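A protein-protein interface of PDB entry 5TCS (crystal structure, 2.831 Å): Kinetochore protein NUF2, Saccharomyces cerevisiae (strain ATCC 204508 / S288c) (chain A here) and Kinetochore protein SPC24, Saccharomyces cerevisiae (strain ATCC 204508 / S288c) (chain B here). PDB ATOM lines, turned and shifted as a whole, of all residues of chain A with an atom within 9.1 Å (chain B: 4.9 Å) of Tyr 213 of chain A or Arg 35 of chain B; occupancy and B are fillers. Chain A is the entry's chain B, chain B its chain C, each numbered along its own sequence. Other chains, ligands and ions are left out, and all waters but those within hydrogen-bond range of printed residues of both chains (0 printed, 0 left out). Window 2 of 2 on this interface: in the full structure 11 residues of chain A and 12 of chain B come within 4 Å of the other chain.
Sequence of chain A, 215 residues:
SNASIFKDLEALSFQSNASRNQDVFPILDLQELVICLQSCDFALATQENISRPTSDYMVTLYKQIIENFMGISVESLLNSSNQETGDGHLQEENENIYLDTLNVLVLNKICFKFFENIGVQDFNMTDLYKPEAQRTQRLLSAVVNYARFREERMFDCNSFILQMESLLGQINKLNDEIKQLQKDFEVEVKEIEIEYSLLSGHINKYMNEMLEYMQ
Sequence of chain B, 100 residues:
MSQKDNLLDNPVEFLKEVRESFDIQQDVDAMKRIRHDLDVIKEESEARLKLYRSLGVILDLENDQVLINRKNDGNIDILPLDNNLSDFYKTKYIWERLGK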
ATOM      1  N   TYR A 206      -1.662 -17.430  32.187  1.00  0.00           N
ATOM      2  CA  TYR A 206      -0.812 -18.561  31.836  1.00  0.00           C
ATOM      3  C   TYR A 206      -1.531 -19.532  30.906  1.00  0.00           C
ATOM      4  O   TYR A 206      -0.952 -19.999  29.920  1.00  0.00           O
ATOM      5  CB  TYR A 206      -0.364 -19.259  33.120  1.00  0.00           C
ATOM      6  CG  TYR A 206       0.265 -20.619  32.943  1.00  0.00           C
ATOM      7  CD1 TYR A 206       1.574 -20.751  32.505  1.00  0.00           C
ATOM      8  CD2 TYR A 206      -0.444 -21.772  33.247  1.00  0.00           C
ATOM      9  CE1 TYR A 206       2.152 -21.990  32.357  1.00  0.00           C
ATOM     10  CE2 TYR A 206       0.123 -23.015  33.103  1.00  0.00           C
ATOM     11  CZ  TYR A 206       1.423 -23.119  32.658  1.00  0.00           C
ATOM     12  OH  TYR A 206       2.000 -24.359  32.513  1.00  0.00           O
ATOM     13  N   MET A 207      -2.790 -19.839  31.194  1.00  0.00           N
ATOM     14  CA  MET A 207      -3.533 -20.807  30.396  1.00  0.00           C
ATOM     15  C   MET A 207      -3.910 -20.237  29.031  1.00  0.00           C
ATOM     16  O   MET A 207      -3.960 -20.965  28.041  1.00  0.00           O
ATOM     17  CB  MET A 207      -4.785 -21.260  31.146  1.00  0.00           C
ATOM     18  CG  MET A 207      -4.489 -22.181  32.321  1.00  0.00           C
ATOM     19  SD  MET A 207      -6.083 -23.016  33.073  1.00  0.00           S
ATOM     20  CE  MET A 207      -6.969 -21.428  33.778  1.00  0.00           C
ATOM     21  N   ASN A 208      -4.173 -18.930  28.983  1.00  0.00           N
ATOM     22  CA  ASN A 208      -4.491 -18.287  27.712  1.00  0.00           C
ATOM     23  C   ASN A 208      -3.287 -18.302  26.779  1.00  0.00           C
ATOM     24  O   ASN A 208      -3.378 -18.769  25.637  1.00  0.00           O
ATOM     25  CB  ASN A 208      -4.964 -16.853  27.951  1.00  0.00           C
ATOM     26  CG  ASN A 208      -6.329 -16.788  28.600  1.00  0.00           C
ATOM     27  OD1 ASN A 208      -7.132 -17.714  28.479  1.00  0.00           O
ATOM     28  ND2 ASN A 208      -6.605 -15.688  29.290  1.00  0.00           N
ATOM     29  N   GLU A 209      -2.147 -17.792  27.249  1.00  0.00           N
ATOM     30  CA  GLU A 209      -0.956 -17.744  26.408  1.00  0.00           C
ATOM     31  C   GLU A 209      -0.560 -19.137  25.940  1.00  0.00           C
ATOM     32  O   GLU A 209      -0.140 -19.318  24.791  1.00  0.00           O
ATOM     33  CB  GLU A 209       0.190 -17.084  27.173  1.00  0.00           C
ATOM     34  CG  GLU A 209       1.434 -16.838  26.334  1.00  0.00           C
ATOM     35  CD  GLU A 209       2.336 -15.768  26.923  1.00  0.00           C
ATOM     36  OE1 GLU A 209       1.967 -15.173  27.958  1.00  0.00           O
ATOM     37  OE2 GLU A 209       3.415 -15.519  26.346  1.00  0.00           O
ATOM     38  N   MET A 210      -0.692 -20.131  26.811  1.00  0.00           N
ATOM     39  CA  MET A 210      -0.355 -21.506  26.468  1.00  0.00           C
ATOM     40  C   MET A 210      -1.258 -22.042  25.361  1.00  0.00           C
ATOM     41  O   MET A 210      -0.773 -22.576  24.365  1.00  0.00           O
ATOM     42  CB  MET A 210      -0.456 -22.396  27.707  1.00  0.00           C
ATOM     43  CG  MET A 210       0.643 -22.155  28.723  1.00  0.00           C
ATOM     44  SD  MET A 210       2.349 -22.937  28.193  1.00  0.00           S
ATOM     45  CE  MET A 210       2.148 -24.693  29.013  1.00  0.00           C
ATOM     46  N   LEU A 211      -2.572 -21.888  25.536  1.00  0.00           N
ATOM     47  CA  LEU A 211      -3.525 -22.441  24.579  1.00  0.00           C
ATOM     48  C   LEU A 211      -3.255 -21.987  23.152  1.00  0.00           C
ATOM     49  O   LEU A 211      -3.697 -22.649  22.207  1.00  0.00           O
ATOM     50  CB  LEU A 211      -4.954 -22.059  24.978  1.00  0.00           C
ATOM     51  CG  LEU A 211      -5.583 -22.905  26.087  1.00  0.00           C
ATOM     52  CD1 LEU A 211      -6.872 -22.268  26.575  1.00  0.00           C
ATOM     53  CD2 LEU A 211      -5.845 -24.327  25.604  1.00  0.00           C
ATOM     54  N   GLU A 212      -2.544 -20.872  22.968  1.00  0.00           N
ATOM     55  CA  GLU A 212      -2.190 -20.441  21.622  1.00  0.00           C
ATOM     56  C   GLU A 212      -1.312 -21.462  20.912  1.00  0.00           C
ATOM     57  O   GLU A 212      -1.234 -21.446  19.679  1.00  0.00           O
ATOM     58  CB  GLU A 212      -1.484 -19.086  21.676  1.00  0.00           C
ATOM     59  CG  GLU A 212      -2.280 -18.017  22.402  1.00  0.00           C
ATOM     60  CD  GLU A 212      -2.068 -16.634  21.823  1.00  0.00           C
ATOM     61  OE1 GLU A 212      -1.205 -15.896  22.340  1.00  0.00           O
ATOM     62  OE2 GLU A 212      -2.765 -16.288  20.844  1.00  0.00           O
ATOM     63  N   TYR A 213      -0.659 -22.352  21.662  1.00  0.00           N
ATOM     64  CA  TYR A 213       0.185 -23.389  21.085  1.00  0.00           C
ATOM     65  C   TYR A 213      -0.503 -24.747  21.021  1.00  0.00           C
ATOM     66  O   TYR A 213      -0.122 -25.576  20.189  1.00  0.00           O
ATOM     67  CB  TYR A 213       1.489 -23.501  21.882  1.00  0.00           C
ATOM     68  CG  TYR A 213       2.271 -22.206  21.896  1.00  0.00           C
ATOM     69  CD1 TYR A 213       1.914 -21.166  22.743  1.00  0.00           C
ATOM     70  CD2 TYR A 213       3.357 -22.019  21.055  1.00  0.00           C
ATOM     71  CE1 TYR A 213       2.619 -19.978  22.753  1.00  0.00           C
ATOM     72  CE2 TYR A 213       4.068 -20.834  21.058  1.00  0.00           C
ATOM     73  CZ  TYR A 213       3.695 -19.818  21.909  1.00  0.00           C
ATOM     74  OH  TYR A 213       4.400 -18.636  21.918  1.00  0.00           O
ATOM     75  N   MET A 214      -1.497 -24.991  21.868  1.00  0.00           N
ATOM     76  CA  MET A 214      -2.415 -26.106  21.655  1.00  0.00           C
ATOM     77  C   MET A 214      -3.277 -25.763  20.438  1.00  0.00           C
ATOM     78  O   MET A 214      -2.966 -24.821  19.713  1.00  0.00           O
ATOM     79  CB  MET A 214      -3.272 -26.364  22.906  1.00  0.00           C
ATOM     80  CG  MET A 214      -2.594 -27.223  23.972  1.00  0.00           C
ATOM     81  SD  MET A 214      -2.381 -26.307  25.683  1.00  0.00           S
ATOM     82  CE  MET A 214      -0.654 -25.481  25.321  1.00  0.00           C
ATOM     83  N   GLN A 215      -4.344 -26.529  20.222  1.00  0.00           N
ATOM     84  CA  GLN A 215      -5.254 -26.345  19.083  1.00  0.00           C
ATOM     85  C   GLN A 215      -4.691 -27.033  17.845  1.00  0.00           C
ATOM     86  O   GLN A 215      -5.418 -27.298  16.887  1.00  0.00           O
ATOM     87  CB  GLN A 215      -5.509 -24.860  18.779  1.00  0.00           C
ATOM     88  CG  GLN A 215      -5.954 -24.023  19.974  1.00  0.00           C
ATOM     89  CD  GLN A 215      -7.401 -24.264  20.352  1.00  0.00           C
ATOM     90  OE1 GLN A 215      -8.185 -24.789  19.559  1.00  0.00           O
ATOM     91  NE2 GLN A 215      -7.765 -23.881  21.569  1.00  0.00           N
ATOM     92  OXT GLN A 215      -3.502 -27.347  17.771  1.00  0.00           O
ATOM     93  N   VAL B  28       5.980 -21.467  28.285  1.00  0.00           N
ATOM     94  CA  VAL B  28       5.728 -21.014  26.918  1.00  0.00           C
ATOM     95  C   VAL B  28       6.927 -21.335  26.033  1.00  0.00           C
ATOM     96  O   VAL B  28       6.793 -21.954  24.968  1.00  0.00           O
ATOM     97  CB  VAL B  28       5.394 -19.511  26.904  1.00  0.00           C
ATOM     98  CG1 VAL B  28       5.508 -18.936  25.494  1.00  0.00           C
ATOM     99  CG2 VAL B  28       3.996 -19.285  27.447  1.00  0.00           C
ATOM    100  N   MET B  31       6.987 -24.831  25.117  1.00  0.00           N
ATOM    101  CA  MET B  31       6.052 -25.166  24.049  1.00  0.00           C
ATOM    102  C   MET B  31       6.648 -24.804  22.696  1.00  0.00           C
ATOM    103  O   MET B  31       6.492 -25.544  21.725  1.00  0.00           O
ATOM    104  CB  MET B  31       4.712 -24.447  24.235  1.00  0.00           C
ATOM    105  CG  MET B  31       3.760 -25.090  25.238  1.00  0.00           C
ATOM    106  SD  MET B  31       3.231 -26.935  24.844  1.00  0.00           S
ATOM    107  CE  MET B  31       3.546 -27.011  22.914  1.00  0.00           C
ATOM    108  N   LYS B  32       7.320 -23.653  22.630  1.00  0.00           N
ATOM    109  CA  LYS B  32       7.989 -23.273  21.390  1.00  0.00           C
ATOM    110  C   LYS B  32       9.028 -24.317  21.002  1.00  0.00           C
ATOM    111  O   LYS B  32       9.090 -24.754  19.845  1.00  0.00           O
ATOM    112  CB  LYS B  32       8.639 -21.898  21.538  1.00  0.00           C
ATOM    113  CG  LYS B  32       7.697 -20.802  21.995  1.00  0.00           C
ATOM    114  CD  LYS B  32       8.255 -19.432  21.650  1.00  0.00           C
ATOM    115  CE  LYS B  32       7.504 -18.316  22.354  1.00  0.00           C
ATOM    116  NZ  LYS B  32       8.409 -17.189  22.712  1.00  0.00           N
ATOM    117  N   ARG B  33       9.856 -24.730  21.966  1.00  0.00           N
ATOM    118  CA  ARG B  33      10.818 -25.797  21.717  1.00  0.00           C
ATOM    119  C   ARG B  33      10.130 -27.043  21.179  1.00  0.00           C
ATOM    120  O   ARG B  33      10.652 -27.715  20.281  1.00  0.00           O
ATOM    121  CB  ARG B  33      11.581 -26.121  23.005  1.00  0.00           C
ATOM    122  CG  ARG B  33      12.830 -25.273  23.213  1.00  0.00           C
ATOM    123  CD  ARG B  33      13.557 -25.622  24.498  1.00  0.00           C
ATOM    124  NE  ARG B  33      13.325 -24.625  25.544  1.00  0.00           N
ATOM    125  CZ  ARG B  33      12.783 -24.865  26.734  1.00  0.00           C
ATOM    126  NH1 ARG B  33      12.413 -26.088  27.084  1.00  0.00           N
ATOM    127  NH2 ARG B  33      12.626 -23.867  27.592  1.00  0.00           N
ATOM    128  N   ILE B  34       8.946 -27.358  21.705  1.00  0.00           N
ATOM    129  CA  ILE B  34       8.262 -28.584  21.308  1.00  0.00           C
ATOM    130  C   ILE B  34       7.739 -28.471  19.881  1.00  0.00           C
ATOM    131  O   ILE B  34       7.851 -29.418  19.094  1.00  0.00           O
ATOM    132  CB  ILE B  34       7.140 -28.913  22.309  1.00  0.00           C
ATOM    133  CG1 ILE B  34       7.763 -29.358  23.637  1.00  0.00           C
ATOM    134  CG2 ILE B  34       6.211 -29.999  21.752  1.00  0.00           C
ATOM    135  CD1 ILE B  34       6.766 -29.687  24.727  1.00  0.00           C
ATOM    136  N   ARG B  35       7.156 -27.325  19.519  1.00  0.00           N
ATOM    137  CA  ARG B  35       6.689 -27.164  18.145  1.00  0.00           C
ATOM    138  C   ARG B  35       7.860 -27.185  17.174  1.00  0.00           C
ATOM    139  O   ARG B  35       7.754 -27.738  16.071  1.00  0.00           O
ATOM    140  CB  ARG B  35       5.892 -25.870  17.987  1.00  0.00           C
ATOM    141  CG  ARG B  35       4.846 -25.947  16.875  1.00  0.00           C
ATOM    142  CD  ARG B  35       4.817 -24.694  16.015  1.00  0.00           C
ATOM    143  NE  ARG B  35       4.770 -23.471  16.814  1.00  0.00           N
ATOM    144  CZ  ARG B  35       3.660 -22.924  17.298  1.00  0.00           C
ATOM    145  NH1 ARG B  35       2.476 -23.484  17.080  1.00  0.00           N
ATOM    146  NH2 ARG B  35       3.734 -21.808  18.009  1.00  0.00           N
ATOM    147  N   HIS B  36       8.990 -26.594  17.567  1.00  0.00           N
ATOM    148  CA  HIS B  36      10.187 -26.682  16.738  1.00  0.00           C
ATOM    149  C   HIS B  36      10.596 -28.136  16.538  1.00  0.00           C
ATOM    150  O   HIS B  36      10.891 -28.560  15.414  1.00  0.00           O
ATOM    151  CB  HIS B  36      11.326 -25.883  17.370  1.00  0.00           C
ATOM    152  CG  HIS B  36      12.572 -25.848  16.539  1.00  0.00           C
ATOM    153  ND1 HIS B  36      13.441 -26.914  16.455  1.00  0.00           N
ATOM    154  CD2 HIS B  36      13.094 -24.875  15.756  1.00  0.00           C
ATOM    155  CE1 HIS B  36      14.444 -26.599  15.655  1.00  0.00           C
ATOM    156  NE2 HIS B  36      14.258 -25.367  15.218  1.00  0.00           N
ATOM    157  N   ASP B  37      10.614 -28.918  17.619  1.00  0.00           N
ATOM    158  CA  ASP B  37      10.938 -30.336  17.494  1.00  0.00           C
ATOM    159  C   ASP B  37       9.980 -31.037  16.540  1.00  0.00           C
ATOM    160  O   ASP B  37      10.406 -31.829  15.690  1.00  0.00           O
ATOM    161  CB  ASP B  37      10.911 -31.009  18.867  1.00  0.00           C
ATOM    162  CG  ASP B  37      12.115 -30.655  19.716  1.00  0.00           C
ATOM    163  OD1 ASP B  37      13.071 -30.059  19.177  1.00  0.00           O
ATOM    164  OD2 ASP B  37      12.108 -30.984  20.921  1.00  0.00           O
ATOM    165  N   LEU B  38       8.681 -30.758  16.663  1.00  0.00           N
ATOM    166  CA  LEU B  38       7.705 -31.383  15.775  1.00  0.00           C
ATOM    167  C   LEU B  38       7.986 -31.037  14.318  1.00  0.00           C
ATOM    168  O   LEU B  38       7.945 -31.913  13.446  1.00  0.00           O
ATOM    169  CB  LEU B  38       6.291 -30.954  16.167  1.00  0.00           C
ATOM    170  CG  LEU B  38       5.774 -31.466  17.516  1.00  0.00           C
ATOM    171  CD1 LEU B  38       4.436 -30.828  17.850  1.00  0.00           C
ATOM    172  CD2 LEU B  38       5.652 -32.982  17.516  1.00  0.00           C
ATOM    173  N   ASP B  39       8.272 -29.764  14.033  1.00  0.00           N
ATOM    174  CA  ASP B  39       8.583 -29.373  12.662  1.00  0.00           C
ATOM    175  C   ASP B  39       9.850 -30.061  12.168  1.00  0.00           C
ATOM    176  O   ASP B  39       9.951 -30.422  10.989  1.00  0.00           O
ATOM    177  CB  ASP B  39       8.723 -27.854  12.571  1.00  0.00           C
ATOM    178  CG  ASP B  39       7.414 -27.134  12.828  1.00  0.00           C
ATOM    179  OD1 ASP B  39       6.350 -27.785  12.755  1.00  0.00           O
ATOM    180  OD2 ASP B  39       7.448 -25.915  13.097  1.00  0.00           O
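Printed residues of chain A that touch a printed residue of chain B: Glu 209, Met 210 and Tyr 213. Hydrophobic or aromatic side chains of chain A within 4 Å of the printed part of chain B: Met 210 and Tyr 213. Along chain A the printed residues that touch a printed residue of chain B span positions 209 to 213. Hydrophobic or aromatic side chains of chain B that line the printed part of chain A: Val 28 and Met 31. Along chain B the printed residues that touch a printed residue of chain A span positions 28 to 35.
Glu 209 of chain A touches Val 28 of chain B (CG to CG2, 3.7 Å). Val 28 of chain B touches Met 210 of chain A. Met 210 of chain A touches Met 31 of chain B. Tyr 213 of chain A touches Val 28 of chain B (OH to CG1, 3.8 Å). Lys 32 of chain B touches Tyr 213 of chain A. NH2 of Arg 35 of chain B touches CD2 of Tyr 213 of chain A, 3.1 Å away.
Arg 35 of chain B touches one residue of chain A. Of the printed residues of chain B, Glu 209 of chain A touches Val 28 (3.7 Å). Printed residues of chain A within 4 Å of Met 31 of chain B: Met 210 (3.9 Å). Of the printed residues of chain B, Met 210 of chain A touches Val 28 (3.9 Å) and Met 31 (3.9 Å). Printed residues of chain A within 4 Å of Val 28 of chain B: Glu 209, Met 210 and Tyr 213. Asn 208 of chain A touches none of the printed residues of chain B. The nearest residue of chain A that does not touch Arg 35 of chain B is Glu 212 of chain A (5.0 Å).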
